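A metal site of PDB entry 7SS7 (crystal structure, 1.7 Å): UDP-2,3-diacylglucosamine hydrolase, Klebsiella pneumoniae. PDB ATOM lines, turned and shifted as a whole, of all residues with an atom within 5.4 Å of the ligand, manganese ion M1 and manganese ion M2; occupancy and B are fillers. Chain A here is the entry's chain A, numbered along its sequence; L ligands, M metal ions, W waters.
O5 of the ligand lies close to O of His 195 (2.9 Å). An oxygen (O3) of the ligand sits close to the guanidinium group (NH1) of Arg 80, at 3.5 Å. O2 of the ligand lies within hydrogen-bond range of N of Trp 46 (3.0 Å).
The side-chain carboxylate (OE1) of Glu 44 lies within salt-bridge range of the guanidinium group (NH2) of Arg 80 (3.4 Å). OH of Tyr 125 is in hydrogen-bond range of OD2 of Asp 116 (2.6 Å). The side-chain carboxylate (OD1) of Asp 41 lies within hydrogen-bond range of the backbone NH (N) of Arg 80, 2.9 Å away. The side-chain carboxylate of Asp 8 sits at hydrogen-bond distance from the backbone NH of His 195 (2.8 Å). O of Val 132 sits at hydrogen-bond distance from NE2 of Gln 138 (2.8 Å).
Ala 45 touches the ligand. Phe 82 touches the ligand (CZ to C9, 3.7 Å). Leu 83 touches the ligand. Tyr 125 touches the ligand (CE1 to C4, 3.6 Å). O of Val 132 touches CL1 of the ligand, 3.8 Å away. Gln 138 touches the ligand (CA to CL1, 3.7 Å). Phe 141 touches the ligand (CE1 to C20, 3.6 Å). Ile 152 touches the ligand (CG2 to F3, 3.7 Å). CB of Ala 153 touches O1 of the ligand, 3.5 Å away. Met 156 touches the ligand. CE of Met 172 touches C5 of the ligand (3.5 Å). Hydrophobic or aromatic side chains that line the ligand: His 10, Ala 45, Phe 82, Leu 83, Tyr 125, Phe 141, Ile 152, Ala 153, Met 156, Met 172, His 195 and His 197. Within 4 Å of the ligand: Asp 8, His 10, Asp 41, Ala 45, Trp 46, Asn 79, Arg 80, Phe 82, Leu 83, His 114, Tyr 125, Val 132, Gln 138, Phe 141, Ile 152, Ala 153, Met 156, Met 172, His 195 and His 197. The nearest printed residue that does not touch the ligand is Ile 137 (4.1 Å).
Five residues have an atom within 4 Å of manganese ion M1: Asp 8, Asp 41, Asn 79, His 114 and His 195.
Within 4 Å of manganese ion M2: Asp 8, His 10, Asp 41 and His 197. The nearest printed residue that does not touch manganese ion M2 is His 195 (4.4 Å).
The side-chain amide oxygen (OD1) of Asn 79 is bound to manganese ion M1 (1.9 Å). Manganese ion M1 is bound by an oxygen (O5) of the ligand, at 2.1 Å. NE2 of His 114 is bound to manganese ion M1, 2.3 Å away. ND1 of His 195 is bound to manganese ion M1. Manganese ion M1 is bound by OD2 of Asp 41 (2.3 Å).
Manganese ion M2 is bound by OD1 of Asp 8, 2.1 Å away. O5 of the ligand binds manganese ion M2 (2.1 Å). Manganese ion M2 is bound by NE2 of His 10 (2.3 Å). Manganese ion M2 is bound by NE2 of His 197 (2.4 Å). Manganese ion M2 is bound by OD2 of Asp 41 (2.4 Å). O4 of the ligand binds manganese ion M2.
Water W2 lies within hydrogen-bond range of an oxygen (O1) of the ligand (2.9 Å) and the backbone carbonyl oxygen of Ala 153 (3.1 Å).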
ATOM      1  N   ASP A   8      14.634 -20.597 -33.707  1.00  0.00           N
ATOM      2  CA  ASP A   8      14.140 -20.629 -32.340  1.00  0.00           C
ATOM      3  C   ASP A   8      12.873 -21.481 -32.195  1.00  0.00           C
ATOM      4  O   ASP A   8      11.926 -21.133 -31.481  1.00  0.00           O
ATOM      5  CB  ASP A   8      13.910 -19.193 -31.839  1.00  0.00           C
ATOM      6  CG  ASP A   8      15.217 -18.424 -31.781  1.00  0.00           C
ATOM      7  OD1 ASP A   8      16.101 -18.852 -31.018  1.00  0.00           O
ATOM      8  OD2 ASP A   8      15.379 -17.425 -32.499  1.00  0.00           O
ATOM      9  N   HIS A  10      13.300 -24.653 -30.904  1.00  0.00           N
ATOM     10  CA  HIS A  10      13.658 -25.366 -29.659  1.00  0.00           C
ATOM     11  C   HIS A  10      12.942 -26.705 -29.573  1.00  0.00           C
ATOM     12  O   HIS A  10      12.361 -27.069 -28.540  1.00  0.00           O
ATOM     13  CB  HIS A  10      13.367 -24.512 -28.417  1.00  0.00           C
ATOM     14  CG  HIS A  10      13.814 -23.094 -28.546  1.00  0.00           C
ATOM     15  ND1 HIS A  10      12.933 -22.049 -28.706  1.00  0.00           N
ATOM     16  CD2 HIS A  10      15.060 -22.537 -28.559  1.00  0.00           C
ATOM     17  CE1 HIS A  10      13.604 -20.921 -28.814  1.00  0.00           C
ATOM     18  NE2 HIS A  10      14.896 -21.190 -28.735  1.00  0.00           N
ATOM     19  N   ASP A  41      18.965 -22.622 -33.287  1.00  0.00           N
ATOM     20  CA  ASP A  41      18.040 -23.066 -32.246  1.00  0.00           C
ATOM     21  C   ASP A  41      16.866 -23.831 -32.844  1.00  0.00           C
ATOM     22  O   ASP A  41      15.707 -23.688 -32.426  1.00  0.00           O
ATOM     23  CB  ASP A  41      17.577 -21.895 -31.366  1.00  0.00           C
ATOM     24  CG  ASP A  41      18.651 -21.444 -30.397  1.00  0.00           C
ATOM     25  OD1 ASP A  41      19.763 -22.018 -30.433  1.00  0.00           O
ATOM     26  OD2 ASP A  41      18.394 -20.515 -29.622  1.00  0.00           O
ATOM     27  N   GLU A  44      16.244 -27.773 -29.002  1.00  0.00           N
ATOM     28  CA  GLU A  44      16.497 -27.226 -27.659  1.00  0.00           C
ATOM     29  C   GLU A  44      17.846 -27.659 -27.112  1.00  0.00           C
ATOM     30  O   GLU A  44      18.405 -26.981 -26.236  1.00  0.00           O
ATOM     31  CB  GLU A  44      15.370 -27.644 -26.699  1.00  0.00           C
ATOM     32  CG  GLU A  44      15.619 -27.308 -25.213  1.00  0.00           C
ATOM     33  CD  GLU A  44      15.718 -25.828 -24.884  1.00  0.00           C
ATOM     34  OE1 GLU A  44      15.956 -25.506 -23.703  1.00  0.00           O
ATOM     35  OE2 GLU A  44      15.543 -24.970 -25.773  1.00  0.00           O
ATOM     36  N   ALA A  45      18.399 -28.771 -27.611  1.00  0.00           N
ATOM     37  CA  ALA A  45      19.691 -29.248 -27.140  1.00  0.00           C
ATOM     38  C   ALA A  45      20.312 -30.088 -28.247  1.00  0.00           C
ATOM     39  O   ALA A  45      19.620 -30.599 -29.135  1.00  0.00           O
ATOM     40  CB  ALA A  45      19.539 -30.077 -25.857  1.00  0.00           C
ATOM     41  N   TRP A  46      21.644 -30.203 -28.222  1.00  0.00           N
ATOM     42  CA  TRP A  46      22.336 -31.120 -29.132  1.00  0.00           C
ATOM     43  C   TRP A  46      23.634 -31.535 -28.479  1.00  0.00           C
ATOM     44  O   TRP A  46      24.410 -30.659 -28.064  1.00  0.00           O
ATOM     45  CB  TRP A  46      22.628 -30.467 -30.493  1.00  0.00           C
ATOM     46  CG  TRP A  46      22.859 -31.466 -31.607  1.00  0.00           C
ATOM     47  CD1 TRP A  46      24.056 -31.949 -32.058  1.00  0.00           C
ATOM     48  CD2 TRP A  46      21.851 -32.057 -32.422  1.00  0.00           C
ATOM     49  NE1 TRP A  46      23.841 -32.829 -33.109  1.00  0.00           N
ATOM     50  CE2 TRP A  46      22.487 -32.907 -33.348  1.00  0.00           C
ATOM     51  CE3 TRP A  46      20.454 -31.965 -32.443  1.00  0.00           C
ATOM     52  CZ2 TRP A  46      21.786 -33.641 -34.307  1.00  0.00           C
ATOM     53  CZ3 TRP A  46      19.748 -32.698 -33.411  1.00  0.00           C
ATOM     54  CH2 TRP A  46      20.414 -33.527 -34.317  1.00  0.00           C
ATOM     55  N   ILE A  47      23.882 -32.835 -28.399  1.00  0.00           N
ATOM     56  CA  ILE A  47      25.121 -33.320 -27.799  1.00  0.00           C
ATOM     57  C   ILE A  47      25.980 -34.094 -28.799  1.00  0.00           C
ATOM     58  O   ILE A  47      26.961 -34.722 -28.399  1.00  0.00           O
ATOM     59  CB  ILE A  47      24.858 -34.166 -26.530  1.00  0.00           C
ATOM     60  CG1 ILE A  47      23.984 -35.389 -26.866  1.00  0.00           C
ATOM     61  CG2 ILE A  47      24.212 -33.296 -25.428  1.00  0.00           C
ATOM     62  CD1 ILE A  47      23.828 -36.372 -25.731  1.00  0.00           C
ATOM     63  N   GLY A  78      22.571 -22.229 -33.741  1.00  0.00           N
ATOM     64  CA  GLY A  78      22.200 -21.417 -32.596  1.00  0.00           C
ATOM     65  C   GLY A  78      23.079 -21.733 -31.384  1.00  0.00           C
ATOM     66  O   GLY A  78      23.966 -22.573 -31.429  1.00  0.00           O
ATOM     67  N   ASN A  79      22.811 -21.029 -30.283  1.00  0.00           N
ATOM     68  CA  ASN A  79      23.531 -21.345 -29.053  1.00  0.00           C
ATOM     69  C   ASN A  79      23.044 -22.661 -28.418  1.00  0.00           C
ATOM     70  O   ASN A  79      23.779 -23.256 -27.628  1.00  0.00           O
ATOM     71  CB  ASN A  79      23.392 -20.200 -28.051  1.00  0.00           C
ATOM     72  CG  ASN A  79      21.964 -19.878 -27.747  1.00  0.00           C
ATOM     73  OD1 ASN A  79      21.245 -19.371 -28.595  1.00  0.00           O
ATOM     74  ND2 ASN A  79      21.527 -20.179 -26.524  1.00  0.00           N
ATOM     75  N   ARG A  80      21.832 -23.113 -28.736  1.00  0.00           N
ATOM     76  CA  ARG A  80      21.395 -24.392 -28.177  1.00  0.00           C
ATOM     77  C   ARG A  80      21.953 -25.570 -28.962  1.00  0.00           C
ATOM     78  O   ARG A  80      22.262 -26.625 -28.376  1.00  0.00           O
ATOM     79  CB  ARG A  80      19.857 -24.500 -28.157  1.00  0.00           C
ATOM     80  CG  ARG A  80      19.154 -23.368 -27.415  1.00  0.00           C
ATOM     81  CD  ARG A  80      19.627 -23.291 -25.951  1.00  0.00           C
ATOM     82  NE  ARG A  80      19.376 -24.545 -25.233  1.00  0.00           N
ATOM     83  CZ  ARG A  80      19.529 -24.674 -23.924  1.00  0.00           C
ATOM     84  NH1 ARG A  80      19.911 -23.654 -23.166  1.00  0.00           N
ATOM     85  NH2 ARG A  80      19.279 -25.849 -23.364  1.00  0.00           N
ATOM     86  N   PHE A  82      24.676 -25.751 -31.314  1.00  0.00           N
ATOM     87  CA  PHE A  82      25.936 -25.491 -31.996  1.00  0.00           C
ATOM     88  C   PHE A  82      26.711 -26.756 -32.347  1.00  0.00           C
ATOM     89  O   PHE A  82      27.633 -26.696 -33.172  1.00  0.00           O
ATOM     90  CB  PHE A  82      26.832 -24.551 -31.149  1.00  0.00           C
ATOM     91  CG  PHE A  82      27.180 -25.081 -29.766  1.00  0.00           C
ATOM     92  CD1 PHE A  82      26.351 -24.817 -28.659  1.00  0.00           C
ATOM     93  CD2 PHE A  82      28.351 -25.797 -29.559  1.00  0.00           C
ATOM     94  CE1 PHE A  82      26.690 -25.291 -27.383  1.00  0.00           C
ATOM     95  CE2 PHE A  82      28.694 -26.278 -28.298  1.00  0.00           C
ATOM     96  CZ  PHE A  82      27.861 -26.022 -27.202  1.00  0.00           C
ATOM     97  N   LEU A  83      26.372 -27.910 -31.762  1.00  0.00           N
ATOM     98  CA  LEU A  83      27.075 -29.149 -32.099  1.00  0.00           C
ATOM     99  C   LEU A  83      26.483 -29.894 -33.285  1.00  0.00           C
ATOM    100  O   LEU A  83      26.969 -30.973 -33.617  1.00  0.00           O
ATOM    101  CB  LEU A  83      27.139 -30.089 -30.897  1.00  0.00           C
ATOM    102  CG  LEU A  83      28.064 -29.651 -29.761  1.00  0.00           C
ATOM    103  CD1 LEU A  83      28.066 -30.707 -28.642  1.00  0.00           C
ATOM    104  CD2 LEU A  83      29.506 -29.393 -30.263  1.00  0.00           C
ATOM    105  N   HIS A 114      22.358 -16.095 -36.392  1.00  0.00           N
ATOM    106  CA  HIS A 114      21.468 -16.464 -35.293  1.00  0.00           C
ATOM    107  C   HIS A 114      21.107 -15.244 -34.460  1.00  0.00           C
ATOM    108  O   HIS A 114      19.950 -15.088 -34.054  1.00  0.00           O
ATOM    109  CB  HIS A 114      22.085 -17.553 -34.394  1.00  0.00           C
ATOM    110  CG  HIS A 114      21.183 -17.941 -33.265  1.00  0.00           C
ATOM    111  ND1 HIS A 114      19.907 -18.435 -33.451  1.00  0.00           N
ATOM    112  CD2 HIS A 114      21.366 -17.897 -31.917  1.00  0.00           C
ATOM    113  CE1 HIS A 114      19.344 -18.672 -32.282  1.00  0.00           C
ATOM    114  NE2 HIS A 114      20.204 -18.355 -31.336  1.00  0.00           N
ATOM    115  N   ASP A 116      23.027 -14.219 -31.533  1.00  0.00           N
ATOM    116  CA  ASP A 116      23.612 -14.134 -30.200  1.00  0.00           C
ATOM    117  C   ASP A 116      24.934 -13.370 -30.200  1.00  0.00           C
ATOM    118  O   ASP A 116      25.289 -12.761 -29.178  1.00  0.00           O
ATOM    119  CB  ASP A 116      23.808 -15.535 -29.598  1.00  0.00           C
ATOM    120  CG  ASP A 116      24.687 -16.425 -30.445  1.00  0.00           C
ATOM    121  OD1 ASP A 116      24.452 -16.561 -31.664  1.00  0.00           O
ATOM    122  OD2 ASP A 116      25.632 -17.013 -29.885  1.00  0.00           O
ATOM    123  N   TYR A 125      28.362 -14.298 -21.341  1.00  0.00           N
ATOM    124  CA  TYR A 125      27.877 -15.212 -22.355  1.00  0.00           C
ATOM    125  C   TYR A 125      28.890 -15.368 -23.481  1.00  0.00           C
ATOM    126  O   TYR A 125      29.166 -16.488 -23.923  1.00  0.00           O
ATOM    127  CB  TYR A 125      26.545 -14.751 -22.921  1.00  0.00           C
ATOM    128  CG  TYR A 125      26.190 -15.561 -24.148  1.00  0.00           C
ATOM    129  CD1 TYR A 125      25.830 -16.890 -24.027  1.00  0.00           C
ATOM    130  CD2 TYR A 125      26.299 -15.020 -25.429  1.00  0.00           C
ATOM    131  CE1 TYR A 125      25.535 -17.657 -25.132  1.00  0.00           C
ATOM    132  CE2 TYR A 125      26.017 -15.791 -26.554  1.00  0.00           C
ATOM    133  CZ  TYR A 125      25.630 -17.103 -26.390  1.00  0.00           C
ATOM    134  OH  TYR A 125      25.345 -17.877 -27.502  1.00  0.00           O
ATOM    135  N   PHE A 128      31.683 -17.743 -22.547  1.00  0.00           N
ATOM    136  CA  PHE A 128      31.203 -19.117 -22.629  1.00  0.00           C
ATOM    137  C   PHE A 128      31.070 -19.575 -24.086  1.00  0.00           C
ATOM    138  O   PHE A 128      31.463 -20.696 -24.435  1.00  0.00           O
ATOM    139  CB  PHE A 128      29.857 -19.223 -21.908  1.00  0.00           C
ATOM    140  CG  PHE A 128      29.124 -20.505 -22.163  1.00  0.00           C
ATOM    141  CD1 PHE A 128      29.426 -21.644 -21.450  1.00  0.00           C
ATOM    142  CD2 PHE A 128      28.123 -20.560 -23.128  1.00  0.00           C
ATOM    143  CE1 PHE A 128      28.750 -22.837 -21.683  1.00  0.00           C
ATOM    144  CE2 PHE A 128      27.449 -21.740 -23.372  1.00  0.00           C
ATOM    145  CZ  PHE A 128      27.761 -22.881 -22.643  1.00  0.00           C
ATOM    146  N   VAL A 132      32.925 -22.942 -25.917  1.00  0.00           N
ATOM    147  CA  VAL A 132      32.262 -24.092 -26.547  1.00  0.00           C
ATOM    148  C   VAL A 132      32.378 -24.076 -28.068  1.00  0.00           C
ATOM    149  O   VAL A 132      32.053 -25.083 -28.705  1.00  0.00           O
ATOM    150  CB  VAL A 132      30.780 -24.251 -26.139  1.00  0.00           C
ATOM    151  CG1 VAL A 132      30.650 -24.465 -24.624  1.00  0.00           C
ATOM    152  CG2 VAL A 132      29.917 -23.065 -26.616  1.00  0.00           C
ATOM    153  N   ILE A 137      37.989 -28.176 -27.782  1.00  0.00           N
ATOM    154  CA  ILE A 137      37.043 -28.445 -26.704  1.00  0.00           C
ATOM    155  C   ILE A 137      35.864 -29.235 -27.243  1.00  0.00           C
ATOM    156  O   ILE A 137      35.418 -30.216 -26.627  1.00  0.00           O
ATOM    157  CB  ILE A 137      36.615 -27.125 -26.031  1.00  0.00           C
ATOM    158  CG1 ILE A 137      37.827 -26.500 -25.344  1.00  0.00           C
ATOM    159  CG2 ILE A 137      35.488 -27.386 -25.028  1.00  0.00           C
ATOM    160  CD1 ILE A 137      37.521 -25.198 -24.597  1.00  0.00           C
ATOM    161  N   GLN A 138      35.343 -28.867 -28.415  1.00  0.00           N
ATOM    162  CA  GLN A 138      34.273 -29.656 -29.012  1.00  0.00           C
ATOM    163  C   GLN A 138      34.713 -31.085 -29.263  1.00  0.00           C
ATOM    164  O   GLN A 138      33.953 -32.029 -29.027  1.00  0.00           O
ATOM    165  CB  GLN A 138      33.792 -29.011 -30.318  1.00  0.00           C
ATOM    166  CG  GLN A 138      33.114 -27.671 -30.128  1.00  0.00           C
ATOM    167  CD  GLN A 138      32.482 -27.193 -31.406  1.00  0.00           C
ATOM    168  OE1 GLN A 138      32.612 -27.841 -32.447  1.00  0.00           O
ATOM    169  NE2 GLN A 138      31.770 -26.058 -31.340  1.00  0.00           N
ATOM    170  N   PHE A 141      34.701 -33.035 -25.965  1.00  0.00           N
ATOM    171  CA  PHE A 141      33.338 -33.322 -25.507  1.00  0.00           C
ATOM    172  C   PHE A 141      32.700 -34.417 -26.349  1.00  0.00           C
ATOM    173  O   PHE A 141      32.118 -35.369 -25.821  1.00  0.00           O
ATOM    174  CB  PHE A 141      32.491 -32.048 -25.551  1.00  0.00           C
ATOM    175  CG  PHE A 141      31.043 -32.285 -25.188  1.00  0.00           C
ATOM    176  CD1 PHE A 141      30.654 -32.333 -23.855  1.00  0.00           C
ATOM    177  CD2 PHE A 141      30.095 -32.490 -26.182  1.00  0.00           C
ATOM    178  CE1 PHE A 141      29.324 -32.552 -23.528  1.00  0.00           C
ATOM    179  CE2 PHE A 141      28.766 -32.718 -25.858  1.00  0.00           C
ATOM    180  CZ  PHE A 141      28.387 -32.750 -24.541  1.00  0.00           C
ATOM    181  N   ILE A 152      25.822 -34.775 -18.663  1.00  0.00           N
ATOM    182  CA  ILE A 152      26.340 -33.415 -18.583  1.00  0.00           C
ATOM    183  C   ILE A 152      25.276 -32.430 -19.015  1.00  0.00           C
ATOM    184  O   ILE A 152      25.039 -31.406 -18.360  1.00  0.00           O
ATOM    185  CB  ILE A 152      27.606 -33.279 -19.440  1.00  0.00           C
ATOM    186  CG1 ILE A 152      28.781 -34.057 -18.838  1.00  0.00           C
ATOM    187  CG2 ILE A 152      27.991 -31.825 -19.633  1.00  0.00           C
ATOM    188  CD1 ILE A 152      29.939 -34.137 -19.785  1.00  0.00           C
ATOM    189  N   ALA A 153      24.585 -32.733 -20.116  1.00  0.00           N
ATOM    190  CA  ALA A 153      23.582 -31.819 -20.645  1.00  0.00           C
ATOM    191  C   ALA A 153      22.397 -31.691 -19.698  1.00  0.00           C
ATOM    192  O   ALA A 153      21.883 -30.581 -19.475  1.00  0.00           O
ATOM    193  CB  ALA A 153      23.124 -32.287 -22.025  1.00  0.00           C
ATOM    194  N   MET A 156      23.437 -29.581 -16.746  1.00  0.00           N
ATOM    195  CA  MET A 156      23.525 -28.147 -17.062  1.00  0.00           C
ATOM    196  C   MET A 156      22.147 -27.504 -17.108  1.00  0.00           C
ATOM    197  O   MET A 156      22.005 -26.322 -16.793  1.00  0.00           O
ATOM    198  CB  MET A 156      24.274 -27.948 -18.380  1.00  0.00           C
ATOM    199  CG  MET A 156      25.794 -28.053 -18.260  1.00  0.00           C
ATOM    200  SD  MET A 156      26.703 -28.093 -19.819  1.00  0.00           S
ATOM    201  CE  MET A 156      26.634 -26.374 -20.308  1.00  0.00           C
ATOM    202  N   MET A 172      18.807 -11.723 -23.099  1.00  0.00           N
ATOM    203  CA  MET A 172      19.592 -10.587 -23.554  1.00  0.00           C
ATOM    204  C   MET A 172      19.088 -10.062 -24.897  1.00  0.00           C
ATOM    205  O   MET A 172      18.502 -10.805 -25.692  1.00  0.00           O
ATOM    206  CB  MET A 172      21.061 -11.007 -23.681  1.00  0.00           C
ATOM    207  CG  MET A 172      21.259 -12.214 -24.598  1.00  0.00           C
ATOM    208  SD  MET A 172      22.664 -13.274 -24.179  1.00  0.00           S
ATOM    209  CE  MET A 172      21.842 -14.858 -24.057  1.00  0.00           C
ATOM    210  N   HIS A 195      17.310 -15.523 -31.943  1.00  0.00           N
ATOM    211  CA  HIS A 195      17.941 -15.513 -30.613  1.00  0.00           C
ATOM    212  C   HIS A 195      17.203 -14.688 -29.566  1.00  0.00           C
ATOM    213  O   HIS A 195      17.022 -15.174 -28.435  1.00  0.00           O
ATOM    214  CB  HIS A 195      19.388 -15.022 -30.645  1.00  0.00           C
ATOM    215  CG  HIS A 195      20.081 -15.206 -29.332  1.00  0.00           C
ATOM    216  ND1 HIS A 195      20.308 -16.445 -28.776  1.00  0.00           N
ATOM    217  CD2 HIS A 195      20.568 -14.304 -28.441  1.00  0.00           C
ATOM    218  CE1 HIS A 195      20.916 -16.305 -27.618  1.00  0.00           C
ATOM    219  NE2 HIS A 195      21.098 -15.016 -27.391  1.00  0.00           N
ATOM    220  N   THR A 196      16.813 -13.452 -29.873  1.00  0.00           N
ATOM    221  CA  THR A 196      16.271 -12.594 -28.827  1.00  0.00           C
ATOM    222  C   THR A 196      14.803 -12.855 -28.550  1.00  0.00           C
ATOM    223  O   THR A 196      14.269 -12.335 -27.564  1.00  0.00           O
ATOM    224  CB  THR A 196      16.470 -11.119 -29.197  1.00  0.00           C
ATOM    225  OG1 THR A 196      15.762 -10.837 -30.404  1.00  0.00           O
ATOM    226  CG2 THR A 196      17.947 -10.831 -29.405  1.00  0.00           C
ATOM    227  N   HIS A 197      14.123 -13.634 -29.396  1.00  0.00           N
ATOM    228  CA  HIS A 197      12.731 -14.010 -29.194  1.00  0.00           C
ATOM    229  C   HIS A 197      11.807 -12.790 -29.112  1.00  0.00           C
ATOM    230  O   HIS A 197      10.812 -12.816 -28.391  1.00  0.00           O
ATOM    231  CB  HIS A 197      12.575 -14.876 -27.937  1.00  0.00           C
ATOM    232  CG  HIS A 197      13.351 -16.157 -27.955  1.00  0.00           C
ATOM    233  ND1 HIS A 197      13.302 -17.076 -26.928  1.00  0.00           N
ATOM    234  CD2 HIS A 197      14.186 -16.682 -28.883  1.00  0.00           C
ATOM    235  CE1 HIS A 197      14.079 -18.106 -27.214  1.00  0.00           C
ATOM    236  NE2 HIS A 197      14.639 -17.887 -28.397  1.00  0.00           N
HETATM  237  C1  LIG L   1      23.141 -26.542 -22.614  1.00  0.00           C
HETATM  238  C2  LIG L   1      23.342 -24.221 -23.163  1.00  0.00           C
HETATM  239  C3  LIG L   1      23.227 -25.851 -24.937  1.00  0.00           C
HETATM  240  C4  LIG L   1      22.694 -19.194 -23.523  1.00  0.00           C
HETATM  241  C5  LIG L   1      20.504 -18.134 -24.238  1.00  0.00           C
HETATM  242  C6  LIG L   1      18.616 -19.637 -24.998  1.00  0.00           C
HETATM  243  C7  LIG L   1      29.561 -28.702 -25.232  1.00  0.00           C
HETATM  244  C8  LIG L   1      28.816 -28.929 -24.100  1.00  0.00           C
HETATM  245  C9  LIG L   1      26.804 -29.164 -25.550  1.00  0.00           C
HETATM  246  C10 LIG L   1      25.449 -28.478 -25.498  1.00  0.00           C
HETATM  247  C11 LIG L   1      25.262 -29.085 -23.158  1.00  0.00           C
HETATM  248  C12 LIG L   1      26.628 -29.751 -23.202  1.00  0.00           C
HETATM  249  C13 LIG L   1      23.126 -26.837 -23.971  1.00  0.00           C
HETATM  250  C14 LIG L   1      23.240 -25.225 -22.210  1.00  0.00           C
HETATM  251  C15 LIG L   1      23.337 -24.537 -24.516  1.00  0.00           C
HETATM  252  C16 LIG L   1      22.998 -21.668 -23.415  1.00  0.00           C
HETATM  253  C17 LIG L   1      21.207 -19.014 -23.189  1.00  0.00           C
HETATM  254  C18 LIG L   1      18.984 -18.347 -24.243  1.00  0.00           C
HETATM  255  C19 LIG L   1      17.942 -19.398 -26.351  1.00  0.00           C
HETATM  256  C20 LIG L   1      29.394 -29.005 -22.842  1.00  0.00           C
HETATM  257  C21 LIG L   1      30.761 -28.847 -22.758  1.00  0.00           C
HETATM  258  C22 LIG L   1      31.535 -28.598 -23.870  1.00  0.00           C
HETATM  259  C23 LIG L   1      30.919 -28.531 -25.116  1.00  0.00           C
HETATM  260  C24 LIG L   1      31.396 -28.933 -21.371  1.00  0.00           C
HETATM  261  F1  LIG L   1      30.860 -27.953 -20.613  1.00  0.00           F
HETATM  262  F2  LIG L   1      32.743 -28.792 -21.491  1.00  0.00           F
HETATM  263  F3  LIG L   1      31.119 -30.134 -20.809  1.00  0.00           F
HETATM  264  N1  LIG L   1      27.402 -29.106 -24.229  1.00  0.00           N
HETATM  265  N2  LIG L   1      24.615 -29.073 -24.463  1.00  0.00           N
HETATM  266  N3  LIG L   1      23.443 -22.858 -22.694  1.00  0.00           N
HETATM  267  N4  LIG L   1      23.153 -20.369 -22.810  1.00  0.00           N
HETATM  268  N5  LIG L   1      18.302 -18.216 -27.126  1.00  0.00           N
HETATM  269  O1  LIG L   1      22.227 -29.282 -23.478  1.00  0.00           O
HETATM  270  O2  LIG L   1      22.500 -28.685 -25.802  1.00  0.00           O
HETATM  271  O3  LIG L   1      22.512 -21.743 -24.500  1.00  0.00           O
HETATM  272  O4  LIG L   1      17.106 -20.155 -26.784  1.00  0.00           O
HETATM  273  O5  LIG L   1      17.679 -17.992 -28.382  1.00  0.00           O
HETATM  274  S1  LIG L   1      23.023 -28.553 -24.448  1.00  0.00           S
HETATM  275 CL1  LIG L   1      31.836 -28.236 -26.590  1.00  0.00          CL
HETATM  276 MN    MN M   1      19.564 -18.581 -29.169  1.00  0.00          MN
HETATM  277 MN    MN M   2      16.290 -19.438 -29.026  1.00  0.00          MN
HETATM  278  O   HOH W   1      16.156 -22.397 -25.251  1.00  0.00           O
HETATM  279  O   HOH W   2      20.352 -28.648 -21.292  1.00  0.00           O
